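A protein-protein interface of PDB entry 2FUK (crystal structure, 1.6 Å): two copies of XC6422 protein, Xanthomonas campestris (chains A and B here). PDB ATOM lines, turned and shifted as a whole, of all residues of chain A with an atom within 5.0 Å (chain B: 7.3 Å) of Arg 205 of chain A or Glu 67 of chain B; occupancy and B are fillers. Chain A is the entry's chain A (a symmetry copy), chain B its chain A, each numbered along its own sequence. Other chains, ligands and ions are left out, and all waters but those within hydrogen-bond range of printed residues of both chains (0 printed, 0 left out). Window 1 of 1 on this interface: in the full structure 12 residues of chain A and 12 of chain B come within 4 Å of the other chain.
Printed residues of chain B that touch a printed residue of chain A: Asp 32, Glu 67, Ile 202, Arg 205 and Gln 209. Of the 13 printed residues of chain A, 5 touch a printed residue of chain B. Hydrophobic or aromatic side chains of chain A within 4 Å of the printed part of chain B: Leu 201 and Ile 202.
CD1 of Leu 201 of chain A touches CB of Asp 32 of chain B, 3.9 Å away. Ile 202 of chain A touches Gln 209 of chain B (CD1 to NE2, 3.9 Å). Gln 209 of chain A touches Ile 202 of chain B (NE2 to CD1, 3.9 Å).
OE1 of Gln 209 of chain B lies close to O of Ala 64 of chain B, at 3.0 Å. The side-chain carboxylate of Glu 67 of chain B lies close to the side-chain amide oxygen of Gln 209 of chain B (2.9 Å). The backbone carbonyl oxygen of Ala 64 of chain A lies close to the side-chain amide oxygen of Gln 209 of chain A, 3.0 Å away. The side-chain carboxylate (OE1) of Glu 67 of chain A lies close to the side-chain amide oxygen (OE1) of Gln 209 of chain A (2.9 Å).
Glu 67 of chain A touches Arg 205 of chain B, and with the chains exchanged Arg 205 of chain A touches Glu 67 of chain B. Ile 202 of chain A touches Gln 209 of chain B, and with the chains exchanged Gln 209 of chain A touches Ile 202 of chain B. Arg 205 of chain B touches its own counterpart, Arg 205 of chain A. Arg 205 of chain A touches Gln 209 of chain B, and with the chains exchanged Gln 209 of chain A touches Arg 205 of chain B. 7 positions are printed for both chains.
NH2 of Arg 205 of chain A is in salt-bridge range of OE1 of Glu 67 of chain B (2.6 Å). NH2 of Arg 205 of chain B lies within salt-bridge range of OE1 of Glu 67 of chain A, 2.6 Å away. The side-chain amide nitrogen (NE2) of Gln 209 of chain A lies close to the guanidinium group (NH1) of Arg 205 of chain B (3.3 Å). The side-chain amide nitrogen (NE2) of Gln 209 of chain B sits close to the guanidinium group (NH1) of Arg 205 of chain A (3.3 Å). NH1 of Arg 205 of chain A sits close to NH1 of Arg 205 of chain B, at 3.3 Å.
Of chain B, only Glu 67 (2.6 Å), Arg 205 (3.1 Å) and Gln 209 (3.3 Å) come within 4 Å of Arg 205 of chain A. Of the printed residues of chain B, Glu 67 of chain A touches Arg 205 (2.6 Å). Printed residues of chain B within 4 Å of Leu 201 of chain A: Asp 32. Gly 206 of chain A touches none of the printed residues of chain B. The nearest residue of chain B that does not touch Arg 205 of chain A is Glu 30 of chain B (5.7 Å). The nearest residue of chain A that does not touch Glu 67 of chain B is Ile 202 of chain A (4.1 Å). The nearest printed residue of chain B that does not touch Ile 202 of chain A is Glu 67 of chain B (4.1 Å).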
ATOM      1  N   MET A  60      18.687 -17.601 -14.955  1.00  0.00           N
ATOM      2  CA  MET A  60      20.139 -17.756 -14.890  1.00  0.00           C
ATOM      3  C   MET A  60      20.498 -18.356 -13.536  1.00  0.00           C
ATOM      4  O   MET A  60      21.462 -19.105 -13.423  1.00  0.00           O
ATOM      5  CB  MET A  60      20.873 -16.428 -15.082  1.00  0.00           C
ATOM      6  CG  MET A  60      22.394 -16.562 -14.958  1.00  0.00           C
ATOM      7  SD  MET A  60      23.128 -17.797 -16.115  1.00  0.00           S
ATOM      8  CE  MET A  60      24.276 -16.743 -17.062  1.00  0.00           C
ATOM      9  N   ALA A  64      22.540 -21.754 -13.179  1.00  0.00           N
ATOM     10  CA  ALA A  64      23.731 -21.810 -12.345  1.00  0.00           C
ATOM     11  C   ALA A  64      23.717 -23.039 -11.442  1.00  0.00           C
ATOM     12  O   ALA A  64      24.742 -23.686 -11.234  1.00  0.00           O
ATOM     13  CB  ALA A  64      23.821 -20.541 -11.508  1.00  0.00           C
ATOM     14  N   GLU A  67      23.897 -26.472 -13.495  1.00  0.00           N
ATOM     15  CA  GLU A  67      25.263 -26.757 -13.926  1.00  0.00           C
ATOM     16  C   GLU A  67      26.083 -27.390 -12.808  1.00  0.00           C
ATOM     17  O   GLU A  67      27.173 -27.917 -13.045  1.00  0.00           O
ATOM     18  CB  GLU A  67      25.941 -25.478 -14.428  1.00  0.00           C
ATOM     19  CG  GLU A  67      25.282 -24.898 -15.676  1.00  0.00           C
ATOM     20  CD  GLU A  67      25.962 -23.640 -16.194  1.00  0.00           C
ATOM     21  OE1 GLU A  67      26.787 -23.058 -15.459  1.00  0.00           O
ATOM     22  OE2 GLU A  67      25.655 -23.223 -17.334  1.00  0.00           O
ATOM     23  N   LEU A 201      24.784 -11.135 -16.103  1.00  0.00           N
ATOM     24  CA  LEU A 201      24.220 -12.444 -15.779  1.00  0.00           C
ATOM     25  C   LEU A 201      25.278 -13.540 -15.653  1.00  0.00           C
ATOM     26  O   LEU A 201      25.137 -14.463 -14.845  1.00  0.00           O
ATOM     27  CB  LEU A 201      23.177 -12.846 -16.828  1.00  0.00           C
ATOM     28  CG  LEU A 201      21.897 -12.003 -16.896  1.00  0.00           C
ATOM     29  CD1 LEU A 201      21.045 -12.480 -18.057  1.00  0.00           C
ATOM     30  CD2 LEU A 201      21.121 -12.112 -15.600  1.00  0.00           C
ATOM     31  N   ILE A 202      26.329 -13.452 -16.460  1.00  0.00           N
ATOM     32  CA  ILE A 202      27.390 -14.448 -16.397  1.00  0.00           C
ATOM     33  C   ILE A 202      28.159 -14.264 -15.088  1.00  0.00           C
ATOM     34  O   ILE A 202      28.604 -15.240 -14.470  1.00  0.00           O
ATOM     35  CB  ILE A 202      28.348 -14.305 -17.597  1.00  0.00           C
ATOM     36  CG1 ILE A 202      29.373 -15.434 -17.583  1.00  0.00           C
ATOM     37  CG2 ILE A 202      29.053 -12.947 -17.552  1.00  0.00           C
ATOM     38  CD1 ILE A 202      30.231 -15.467 -18.830  1.00  0.00           C
ATOM     39  N   ASP A 203      28.306 -13.013 -14.661  1.00  0.00           N
ATOM     40  CA  ASP A 203      29.003 -12.723 -13.415  1.00  0.00           C
ATOM     41  C   ASP A 203      28.158 -13.235 -12.257  1.00  0.00           C
ATOM     42  O   ASP A 203      28.686 -13.714 -11.256  1.00  0.00           O
ATOM     43  CB  ASP A 203      29.221 -11.223 -13.237  1.00  0.00           C
ATOM     44  CG  ASP A 203      30.041 -10.617 -14.348  1.00  0.00           C
ATOM     45  OD1 ASP A 203      29.524 -10.507 -15.484  1.00  0.00           O
ATOM     46  OD2 ASP A 203      31.202 -10.250 -14.081  1.00  0.00           O
ATOM     47  N   LEU A 204      26.841 -13.100 -12.392  1.00  0.00           N
ATOM     48  CA  LEU A 204      25.914 -13.564 -11.370  1.00  0.00           C
ATOM     49  C   LEU A 204      26.053 -15.081 -11.240  1.00  0.00           C
ATOM     50  O   LEU A 204      26.085 -15.624 -10.136  1.00  0.00           O
ATOM     51  CB  LEU A 204      24.478 -13.191 -11.756  1.00  0.00           C
ATOM     52  CG  LEU A 204      23.358 -13.823 -10.924  1.00  0.00           C
ATOM     53  CD1 LEU A 204      23.440 -13.350  -9.476  1.00  0.00           C
ATOM     54  CD2 LEU A 204      22.005 -13.467 -11.545  1.00  0.00           C
ATOM     55  N   ARG A 205      26.130 -15.757 -12.380  1.00  0.00           N
ATOM     56  CA  ARG A 205      26.282 -17.208 -12.403  1.00  0.00           C
ATOM     57  C   ARG A 205      27.528 -17.607 -11.615  1.00  0.00           C
ATOM     58  O   ARG A 205      27.487 -18.514 -10.792  1.00  0.00           O
ATOM     59  CB  ARG A 205      26.420 -17.702 -13.850  1.00  0.00           C
ATOM     60  CG  ARG A 205      26.476 -19.219 -14.000  1.00  0.00           C
ATOM     61  CD  ARG A 205      26.948 -19.602 -15.392  1.00  0.00           C
ATOM     62  NE  ARG A 205      28.353 -19.251 -15.580  1.00  0.00           N
ATOM     63  CZ  ARG A 205      28.981 -19.241 -16.755  1.00  0.00           C
ATOM     64  NH1 ARG A 205      30.264 -18.912 -16.808  1.00  0.00           N
ATOM     65  NH2 ARG A 205      28.329 -19.544 -17.872  1.00  0.00           N
ATOM     66  N   GLY A 206      28.639 -16.923 -11.879  1.00  0.00           N
ATOM     67  CA  GLY A 206      29.878 -17.231 -11.187  1.00  0.00           C
ATOM     68  C   GLY A 206      29.805 -17.019  -9.687  1.00  0.00           C
ATOM     69  O   GLY A 206      30.310 -17.830  -8.909  1.00  0.00           O
ATOM     70  N   ALA A 207      29.174 -15.921  -9.277  1.00  0.00           N
ATOM     71  CA  ALA A 207      29.050 -15.609  -7.863  1.00  0.00           C
ATOM     72  C   ALA A 207      28.233 -16.669  -7.142  1.00  0.00           C
ATOM     73  O   ALA A 207      28.564 -17.060  -6.024  1.00  0.00           O
ATOM     74  CB  ALA A 207      28.406 -14.241  -7.681  1.00  0.00           C
ATOM     75  N   LEU A 208      27.165 -17.129  -7.784  1.00  0.00           N
ATOM     76  CA  LEU A 208      26.293 -18.140  -7.195  1.00  0.00           C
ATOM     77  C   LEU A 208      27.018 -19.468  -7.058  1.00  0.00           C
ATOM     78  O   LEU A 208      26.991 -20.103  -6.005  1.00  0.00           O
ATOM     79  CB  LEU A 208      25.046 -18.340  -8.064  1.00  0.00           C
ATOM     80  CG  LEU A 208      23.963 -17.259  -8.076  1.00  0.00           C
ATOM     81  CD1 LEU A 208      23.007 -17.514  -9.240  1.00  0.00           C
ATOM     82  CD2 LEU A 208      23.203 -17.267  -6.750  1.00  0.00           C
ATOM     83  N   GLN A 209      27.676 -19.882  -8.136  1.00  0.00           N
ATOM     84  CA  GLN A 209      28.382 -21.151  -8.136  1.00  0.00           C
ATOM     85  C   GLN A 209      29.535 -21.172  -7.144  1.00  0.00           C
ATOM     86  O   GLN A 209      29.697 -22.134  -6.392  1.00  0.00           O
ATOM     87  CB  GLN A 209      28.847 -21.486  -9.557  1.00  0.00           C
ATOM     88  CG  GLN A 209      27.674 -21.891 -10.441  1.00  0.00           C
ATOM     89  CD  GLN A 209      28.033 -22.194 -11.884  1.00  0.00           C
ATOM     90  OE1 GLN A 209      27.231 -22.778 -12.611  1.00  0.00           O
ATOM     91  NE2 GLN A 209      29.227 -21.791 -12.310  1.00  0.00           N
ATOM     92  N   HIS A 210      30.326 -20.111  -7.111  1.00  0.00           N
ATOM     93  CA  HIS A 210      31.432 -20.084  -6.167  1.00  0.00           C
ATOM     94  C   HIS A 210      30.909 -19.989  -4.740  1.00  0.00           C
ATOM     95  O   HIS A 210      31.497 -20.555  -3.811  1.00  0.00           O
ATOM     96  CB  HIS A 210      32.350 -18.900  -6.444  1.00  0.00           C
ATOM     97  CG  HIS A 210      33.524 -18.834  -5.522  1.00  0.00           C
ATOM     98  ND1 HIS A 210      34.535 -19.772  -5.542  1.00  0.00           N
ATOM     99  CD2 HIS A 210      33.827 -17.973  -4.521  1.00  0.00           C
ATOM    100  CE1 HIS A 210      35.411 -19.491  -4.594  1.00  0.00           C
ATOM    101  NE2 HIS A 210      35.003 -18.404  -3.959  1.00  0.00           N
ATOM    102  N   LEU B  28      24.555 -19.111 -32.585  1.00  0.00           N
ATOM    103  CA  LEU B  28      24.586 -17.679 -32.294  1.00  0.00           C
ATOM    104  C   LEU B  28      24.989 -17.431 -30.841  1.00  0.00           C
ATOM    105  O   LEU B  28      24.880 -18.317 -29.996  1.00  0.00           O
ATOM    106  CB  LEU B  28      23.221 -17.053 -32.588  1.00  0.00           C
ATOM    107  CG  LEU B  28      22.890 -16.986 -34.078  1.00  0.00           C
ATOM    108  CD1 LEU B  28      21.465 -16.496 -34.286  1.00  0.00           C
ATOM    109  CD2 LEU B  28      23.886 -16.067 -34.764  1.00  0.00           C
ATOM    110  N   PRO B  29      25.469 -16.220 -30.533  1.00  0.00           N
ATOM    111  CA  PRO B  29      25.886 -15.903 -29.164  1.00  0.00           C
ATOM    112  C   PRO B  29      24.779 -15.963 -28.124  1.00  0.00           C
ATOM    113  O   PRO B  29      23.588 -15.929 -28.452  1.00  0.00           O
ATOM    114  CB  PRO B  29      26.484 -14.507 -29.303  1.00  0.00           C
ATOM    115  CG  PRO B  29      25.711 -13.929 -30.399  1.00  0.00           C
ATOM    116  CD  PRO B  29      25.641 -15.050 -31.405  1.00  0.00           C
ATOM    117  N   GLU B  30      25.188 -16.063 -26.867  1.00  0.00           N
ATOM    118  CA  GLU B  30      24.259 -16.123 -25.746  1.00  0.00           C
ATOM    119  C   GLU B  30      23.407 -14.861 -25.716  1.00  0.00           C
ATOM    120  O   GLU B  30      23.903 -13.756 -25.972  1.00  0.00           O
ATOM    121  CB  GLU B  30      25.046 -16.233 -24.437  1.00  0.00           C
ATOM    122  CG  GLU B  30      24.201 -16.314 -23.167  1.00  0.00           C
ATOM    123  CD  GLU B  30      23.815 -17.739 -22.811  1.00  0.00           C
ATOM    124  OE1 GLU B  30      23.003 -18.350 -23.540  1.00  0.00           O
ATOM    125  OE2 GLU B  30      24.336 -18.258 -21.798  1.00  0.00           O
ATOM    126  N   PRO B  31      22.106 -15.006 -25.421  1.00  0.00           N
ATOM    127  CA  PRO B  31      21.242 -13.824 -25.367  1.00  0.00           C
ATOM    128  C   PRO B  31      21.579 -13.034 -24.101  1.00  0.00           C
ATOM    129  O   PRO B  31      22.098 -13.598 -23.129  1.00  0.00           O
ATOM    130  CB  PRO B  31      19.835 -14.424 -25.309  1.00  0.00           C
ATOM    131  CG  PRO B  31      19.996 -15.758 -25.979  1.00  0.00           C
ATOM    132  CD  PRO B  31      21.300 -16.239 -25.401  1.00  0.00           C
ATOM    133  N   ASP B  32      21.303 -11.732 -24.122  1.00  0.00           N
ATOM    134  CA  ASP B  32      21.552 -10.852 -22.981  1.00  0.00           C
ATOM    135  C   ASP B  32      23.026 -10.688 -22.613  1.00  0.00           C
ATOM    136  O   ASP B  32      23.365 -10.469 -21.452  1.00  0.00           O
ATOM    137  CB  ASP B  32      20.771 -11.342 -21.762  1.00  0.00           C
ATOM    138  CG  ASP B  32      19.279 -11.386 -22.011  1.00  0.00           C
ATOM    139  OD1 ASP B  32      18.668 -10.314 -22.233  1.00  0.00           O
ATOM    140  OD2 ASP B  32      18.715 -12.493 -21.992  1.00  0.00           O
ATOM    141  N   VAL B  33      23.889 -10.802 -23.616  1.00  0.00           N
ATOM    142  CA  VAL B  33      25.328 -10.641 -23.450  1.00  0.00           C
ATOM    143  C   VAL B  33      25.802  -9.728 -24.579  1.00  0.00           C
ATOM    144  O   VAL B  33      25.308  -9.812 -25.708  1.00  0.00           O
ATOM    145  CB  VAL B  33      26.065 -12.003 -23.541  1.00  0.00           C
ATOM    146  CG1 VAL B  33      27.569 -11.799 -23.590  1.00  0.00           C
ATOM    147  CG2 VAL B  33      25.689 -12.865 -22.351  1.00  0.00           C
ATOM    148  N   ALA B  34      26.741  -8.844 -24.267  1.00  0.00           N
ATOM    149  CA  ALA B  34      27.283  -7.925 -25.261  1.00  0.00           C
ATOM    150  C   ALA B  34      27.849  -8.710 -26.442  1.00  0.00           C
ATOM    151  O   ALA B  34      28.735  -9.557 -26.275  1.00  0.00           O
ATOM    152  CB  ALA B  34      28.370  -7.065 -24.635  1.00  0.00           C
ATOM    153  N   MET B  60      31.260 -27.718 -25.550  1.00  0.00           N
ATOM    154  CA  MET B  60      31.414 -26.876 -24.365  1.00  0.00           C
ATOM    155  C   MET B  60      32.349 -25.724 -24.712  1.00  0.00           C
ATOM    156  O   MET B  60      32.203 -24.625 -24.188  1.00  0.00           O
ATOM    157  CB  MET B  60      31.968 -27.653 -23.170  1.00  0.00           C
ATOM    158  CG  MET B  60      32.192 -26.774 -21.936  1.00  0.00           C
ATOM    159  SD  MET B  60      30.681 -25.871 -21.384  1.00  0.00           S
ATOM    160  CE  MET B  60      30.496 -26.514 -19.686  1.00  0.00           C
ATOM    161  N   ALA B  61      33.312 -25.977 -25.594  1.00  0.00           N
ATOM    162  CA  ALA B  61      34.224 -24.918 -26.002  1.00  0.00           C
ATOM    163  C   ALA B  61      33.393 -23.898 -26.768  1.00  0.00           C
ATOM    164  O   ALA B  61      33.590 -22.692 -26.628  1.00  0.00           O
ATOM    165  CB  ALA B  61      35.335 -25.476 -26.900  1.00  0.00           C
ATOM    166  N   ALA B  62      32.457 -24.393 -27.572  1.00  0.00           N
ATOM    167  CA  ALA B  62      31.600 -23.514 -28.354  1.00  0.00           C
ATOM    168  C   ALA B  62      30.718 -22.686 -27.430  1.00  0.00           C
ATOM    169  O   ALA B  62      30.562 -21.484 -27.627  1.00  0.00           O
ATOM    170  CB  ALA B  62      30.736 -24.338 -29.317  1.00  0.00           C
ATOM    171  N   ARG B  63      30.156 -23.334 -26.415  1.00  0.00           N
ATOM    172  CA  ARG B  63      29.283 -22.658 -25.465  1.00  0.00           C
ATOM    173  C   ARG B  63      30.042 -21.593 -24.691  1.00  0.00           C
ATOM    174  O   ARG B  63      29.518 -20.515 -24.430  1.00  0.00           O
ATOM    175  CB  ARG B  63      28.689 -23.668 -24.484  1.00  0.00           C
ATOM    176  CG  ARG B  63      27.592 -23.095 -23.601  1.00  0.00           C
ATOM    177  CD  ARG B  63      27.048 -24.167 -22.679  1.00  0.00           C
ATOM    178  NE  ARG B  63      26.706 -25.393 -23.398  1.00  0.00           N
ATOM    179  CZ  ARG B  63      26.379 -26.533 -22.798  1.00  0.00           C
ATOM    180  NH1 ARG B  63      26.347 -26.590 -21.473  1.00  0.00           N
ATOM    181  NH2 ARG B  63      26.093 -27.613 -23.517  1.00  0.00           N
ATOM    182  N   ALA B  64      31.276 -21.911 -24.314  1.00  0.00           N
ATOM    183  CA  ALA B  64      32.115 -20.987 -23.567  1.00  0.00           C
ATOM    184  C   ALA B  64      32.313 -19.680 -24.328  1.00  0.00           C
ATOM    185  O   ALA B  64      32.305 -18.598 -23.743  1.00  0.00           O
ATOM    186  CB  ALA B  64      33.462 -21.642 -23.286  1.00  0.00           C
ATOM    187  N   LEU B  65      32.492 -19.785 -25.641  1.00  0.00           N
ATOM    188  CA  LEU B  65      32.695 -18.607 -26.477  1.00  0.00           C
ATOM    189  C   LEU B  65      31.384 -17.874 -26.741  1.00  0.00           C
ATOM    190  O   LEU B  65      31.357 -16.648 -26.768  1.00  0.00           O
ATOM    191  CB  LEU B  65      33.344 -19.011 -27.795  1.00  0.00           C
ATOM    192  CG  LEU B  65      34.742 -19.621 -27.660  1.00  0.00           C
ATOM    193  CD1 LEU B  65      35.225 -20.095 -29.026  1.00  0.00           C
ATOM    194  CD2 LEU B  65      35.691 -18.597 -27.081  1.00  0.00           C
ATOM    195  N   ARG B  66      30.303 -18.623 -26.936  1.00  0.00           N
ATOM    196  CA  ARG B  66      28.996 -18.015 -27.177  1.00  0.00           C
ATOM    197  C   ARG B  66      28.583 -17.155 -25.985  1.00  0.00           C
ATOM    198  O   ARG B  66      27.980 -16.089 -26.145  1.00  0.00           O
ATOM    199  CB  ARG B  66      27.937 -19.101 -27.390  1.00  0.00           C
ATOM    200  CG  ARG B  66      28.151 -19.950 -28.627  1.00  0.00           C
ATOM    201  CD  ARG B  66      27.222 -21.164 -28.637  1.00  0.00           C
ATOM    202  NE  ARG B  66      25.818 -20.790 -28.796  1.00  0.00           N
ATOM    203  CZ  ARG B  66      24.808 -21.654 -28.723  1.00  0.00           C
ATOM    204  NH1 ARG B  66      23.560 -21.233 -28.887  1.00  0.00           N
ATOM    205  NH2 ARG B  66      25.042 -22.937 -28.471  1.00  0.00           N
ATOM    206  N   GLU B  67      28.906 -17.626 -24.787  1.00  0.00           N
ATOM    207  CA  GLU B  67      28.556 -16.907 -23.565  1.00  0.00           C
ATOM    208  C   GLU B  67      29.323 -15.595 -23.447  1.00  0.00           C
ATOM    209  O   GLU B  67      28.993 -14.743 -22.618  1.00  0.00           O
ATOM    210  CB  GLU B  67      28.811 -17.787 -22.337  1.00  0.00           C
ATOM    211  CG  GLU B  67      27.924 -19.028 -22.293  1.00  0.00           C
ATOM    212  CD  GLU B  67      28.154 -19.897 -21.066  1.00  0.00           C
ATOM    213  OE1 GLU B  67      29.169 -19.692 -20.367  1.00  0.00           O
ATOM    214  OE2 GLU B  67      27.325 -20.800 -20.810  1.00  0.00           O
ATOM    215  N   LEU B  68      30.347 -15.435 -24.278  1.00  0.00           N
ATOM    216  CA  LEU B  68      31.133 -14.211 -24.284  1.00  0.00           C
ATOM    217  C   LEU B  68      30.676 -13.293 -25.419  1.00  0.00           C
ATOM    218  O   LEU B  68      31.290 -12.255 -25.669  1.00  0.00           O
ATOM    219  CB  LEU B  68      32.618 -14.528 -24.445  1.00  0.00           C
ATOM    220  CG  LEU B  68      33.257 -15.328 -23.309  1.00  0.00           C
ATOM    221  CD1 LEU B  68      34.730 -15.508 -23.601  1.00  0.00           C
ATOM    222  CD2 LEU B  68      33.057 -14.604 -21.992  1.00  0.00           C
ATOM    223  N   GLY B  69      29.605 -13.694 -26.102  1.00  0.00           N
ATOM    224  CA  GLY B  69      29.060 -12.905 -27.199  1.00  0.00           C
ATOM    225  C   GLY B  69      29.635 -13.221 -28.570  1.00  0.00           C
ATOM    226  O   GLY B  69      29.458 -12.464 -29.526  1.00  0.00           O
ATOM    227  N   ILE B  70      30.318 -14.354 -28.675  1.00  0.00           N
ATOM    228  CA  ILE B  70      30.932 -14.759 -29.931  1.00  0.00           C
ATOM    229  C   ILE B  70      30.077 -15.767 -30.697  1.00  0.00           C
ATOM    230  O   ILE B  70      29.529 -16.695 -30.111  1.00  0.00           O
ATOM    231  CB  ILE B  70      32.329 -15.378 -29.663  1.00  0.00           C
ATOM    232  CG1 ILE B  70      33.261 -14.308 -29.084  1.00  0.00           C
ATOM    233  CG2 ILE B  70      32.908 -15.972 -30.944  1.00  0.00           C
ATOM    234  CD1 ILE B  70      34.582 -14.853 -28.563  1.00  0.00           C
ATOM    235  N   VAL B  72      29.673 -18.873 -32.983  1.00  0.00           N
ATOM    236  CA  VAL B  72      30.548 -20.018 -33.179  1.00  0.00           C
ATOM    237  C   VAL B  72      30.139 -20.954 -34.300  1.00  0.00           C
ATOM    238  O   VAL B  72      28.964 -21.255 -34.480  1.00  0.00           O
ATOM    239  CB  VAL B  72      30.687 -20.829 -31.870  1.00  0.00           C
ATOM    240  CG1 VAL B  72      31.225 -19.930 -30.770  1.00  0.00           C
ATOM    241  CG2 VAL B  72      29.350 -21.397 -31.455  1.00  0.00           C
ATOM    242  N   ILE B 202      32.836 -27.927 -16.869  1.00  0.00           N
ATOM    243  CA  ILE B 202      32.540 -26.604 -16.336  1.00  0.00           C
ATOM    244  C   ILE B 202      33.857 -25.896 -16.021  1.00  0.00           C
ATOM    245  O   ILE B 202      33.982 -24.676 -16.196  1.00  0.00           O
ATOM    246  CB  ILE B 202      31.676 -26.706 -15.063  1.00  0.00           C
ATOM    247  CG1 ILE B 202      31.270 -25.312 -14.595  1.00  0.00           C
ATOM    248  CG2 ILE B 202      32.448 -27.433 -13.959  1.00  0.00           C
ATOM    249  CD1 ILE B 202      30.270 -25.340 -13.459  1.00  0.00           C
ATOM    250  N   ARG B 205      35.262 -24.670 -19.215  1.00  0.00           N
ATOM    251  CA  ARG B 205      34.566 -23.451 -19.615  1.00  0.00           C
ATOM    252  C   ARG B 205      35.209 -22.245 -18.934  1.00  0.00           C
ATOM    253  O   ARG B 205      35.486 -21.236 -19.573  1.00  0.00           O
ATOM    254  CB  ARG B 205      33.087 -23.531 -19.213  1.00  0.00           C
ATOM    255  CG  ARG B 205      32.238 -22.352 -19.680  1.00  0.00           C
ATOM    256  CD  ARG B 205      30.899 -22.341 -18.963  1.00  0.00           C
ATOM    257  NE  ARG B 205      31.069 -22.018 -17.549  1.00  0.00           N
ATOM    258  CZ  ARG B 205      30.125 -22.163 -16.620  1.00  0.00           C
ATOM    259  NH1 ARG B 205      30.388 -21.831 -15.363  1.00  0.00           N
ATOM    260  NH2 ARG B 205      28.931 -22.649 -16.940  1.00  0.00           N
ATOM    261  N   GLY B 206      35.436 -22.356 -17.627  1.00  0.00           N
ATOM    262  CA  GLY B 206      36.038 -21.262 -16.886  1.00  0.00           C
ATOM    263  C   GLY B 206      37.436 -20.908 -17.355  1.00  0.00           C
ATOM    264  O   GLY B 206      37.785 -19.731 -17.468  1.00  0.00           O
ATOM    265  N   GLN B 209      37.166 -19.070 -20.773  1.00  0.00           N
ATOM    266  CA  GLN B 209      36.643 -17.722 -20.631  1.00  0.00           C
ATOM    267  C   GLN B 209      37.633 -16.785 -19.955  1.00  0.00           C
ATOM    268  O   GLN B 209      37.847 -15.662 -20.414  1.00  0.00           O
ATOM    269  CB  GLN B 209      35.301 -17.762 -19.892  1.00  0.00           C
ATOM    270  CG  GLN B 209      34.200 -18.329 -20.779  1.00  0.00           C
ATOM    271  CD  GLN B 209      32.842 -18.454 -20.114  1.00  0.00           C
ATOM    272  OE1 GLN B 209      31.835 -18.643 -20.795  1.00  0.00           O
ATOM    273  NE2 GLN B 209      32.804 -18.362 -18.788  1.00  0.00           N
ATOM    274  N   ARG B 213      39.337 -13.666 -22.036  1.00  0.00           N
ATOM    275  CA  ARG B 213      38.668 -12.439 -21.592  1.00  0.00           C
ATOM    276  C   ARG B 213      39.265 -11.128 -22.097  1.00  0.00           C
ATOM    277  O   ARG B 213      38.564 -10.287 -22.674  1.00  0.00           O
ATOM    278  CB  ARG B 213      38.639 -12.391 -20.066  1.00  0.00           C
ATOM    279  CG  ARG B 213      38.148 -11.070 -19.500  1.00  0.00           C
ATOM    280  CD  ARG B 213      36.662 -10.932 -19.706  1.00  0.00           C
ATOM    281  NE  ARG B 213      35.921 -11.931 -18.946  1.00  0.00           N
ATOM    282  CZ  ARG B 213      34.642 -12.228 -19.149  1.00  0.00           C
ATOM    283  NH1 ARG B 213      34.051 -13.150 -18.403  1.00  0.00           N
ATOM    284  NH2 ARG B 213      33.960 -11.627 -20.118  1.00  0.00           N
ATOM    285  N   PRO B 220      32.594  -6.353 -22.512  1.00  0.00           N
ATOM    286  CA  PRO B 220      31.380  -7.058 -22.087  1.00  0.00           C
ATOM    287  C   PRO B 220      30.472  -6.184 -21.227  1.00  0.00           C
ATOM    288  O   PRO B 220      31.003  -5.305 -20.504  1.00  0.00           O
ATOM    289  CB  PRO B 220      31.924  -8.259 -21.318  1.00  0.00           C
ATOM    290  CG  PRO B 220      33.242  -7.767 -20.796  1.00  0.00           C
ATOM    291  CD  PRO B 220      33.797  -7.011 -21.973  1.00  0.00           C
ATOM    292  OXT PRO B 220      29.242  -6.402 -21.291  1.00  0.00           O
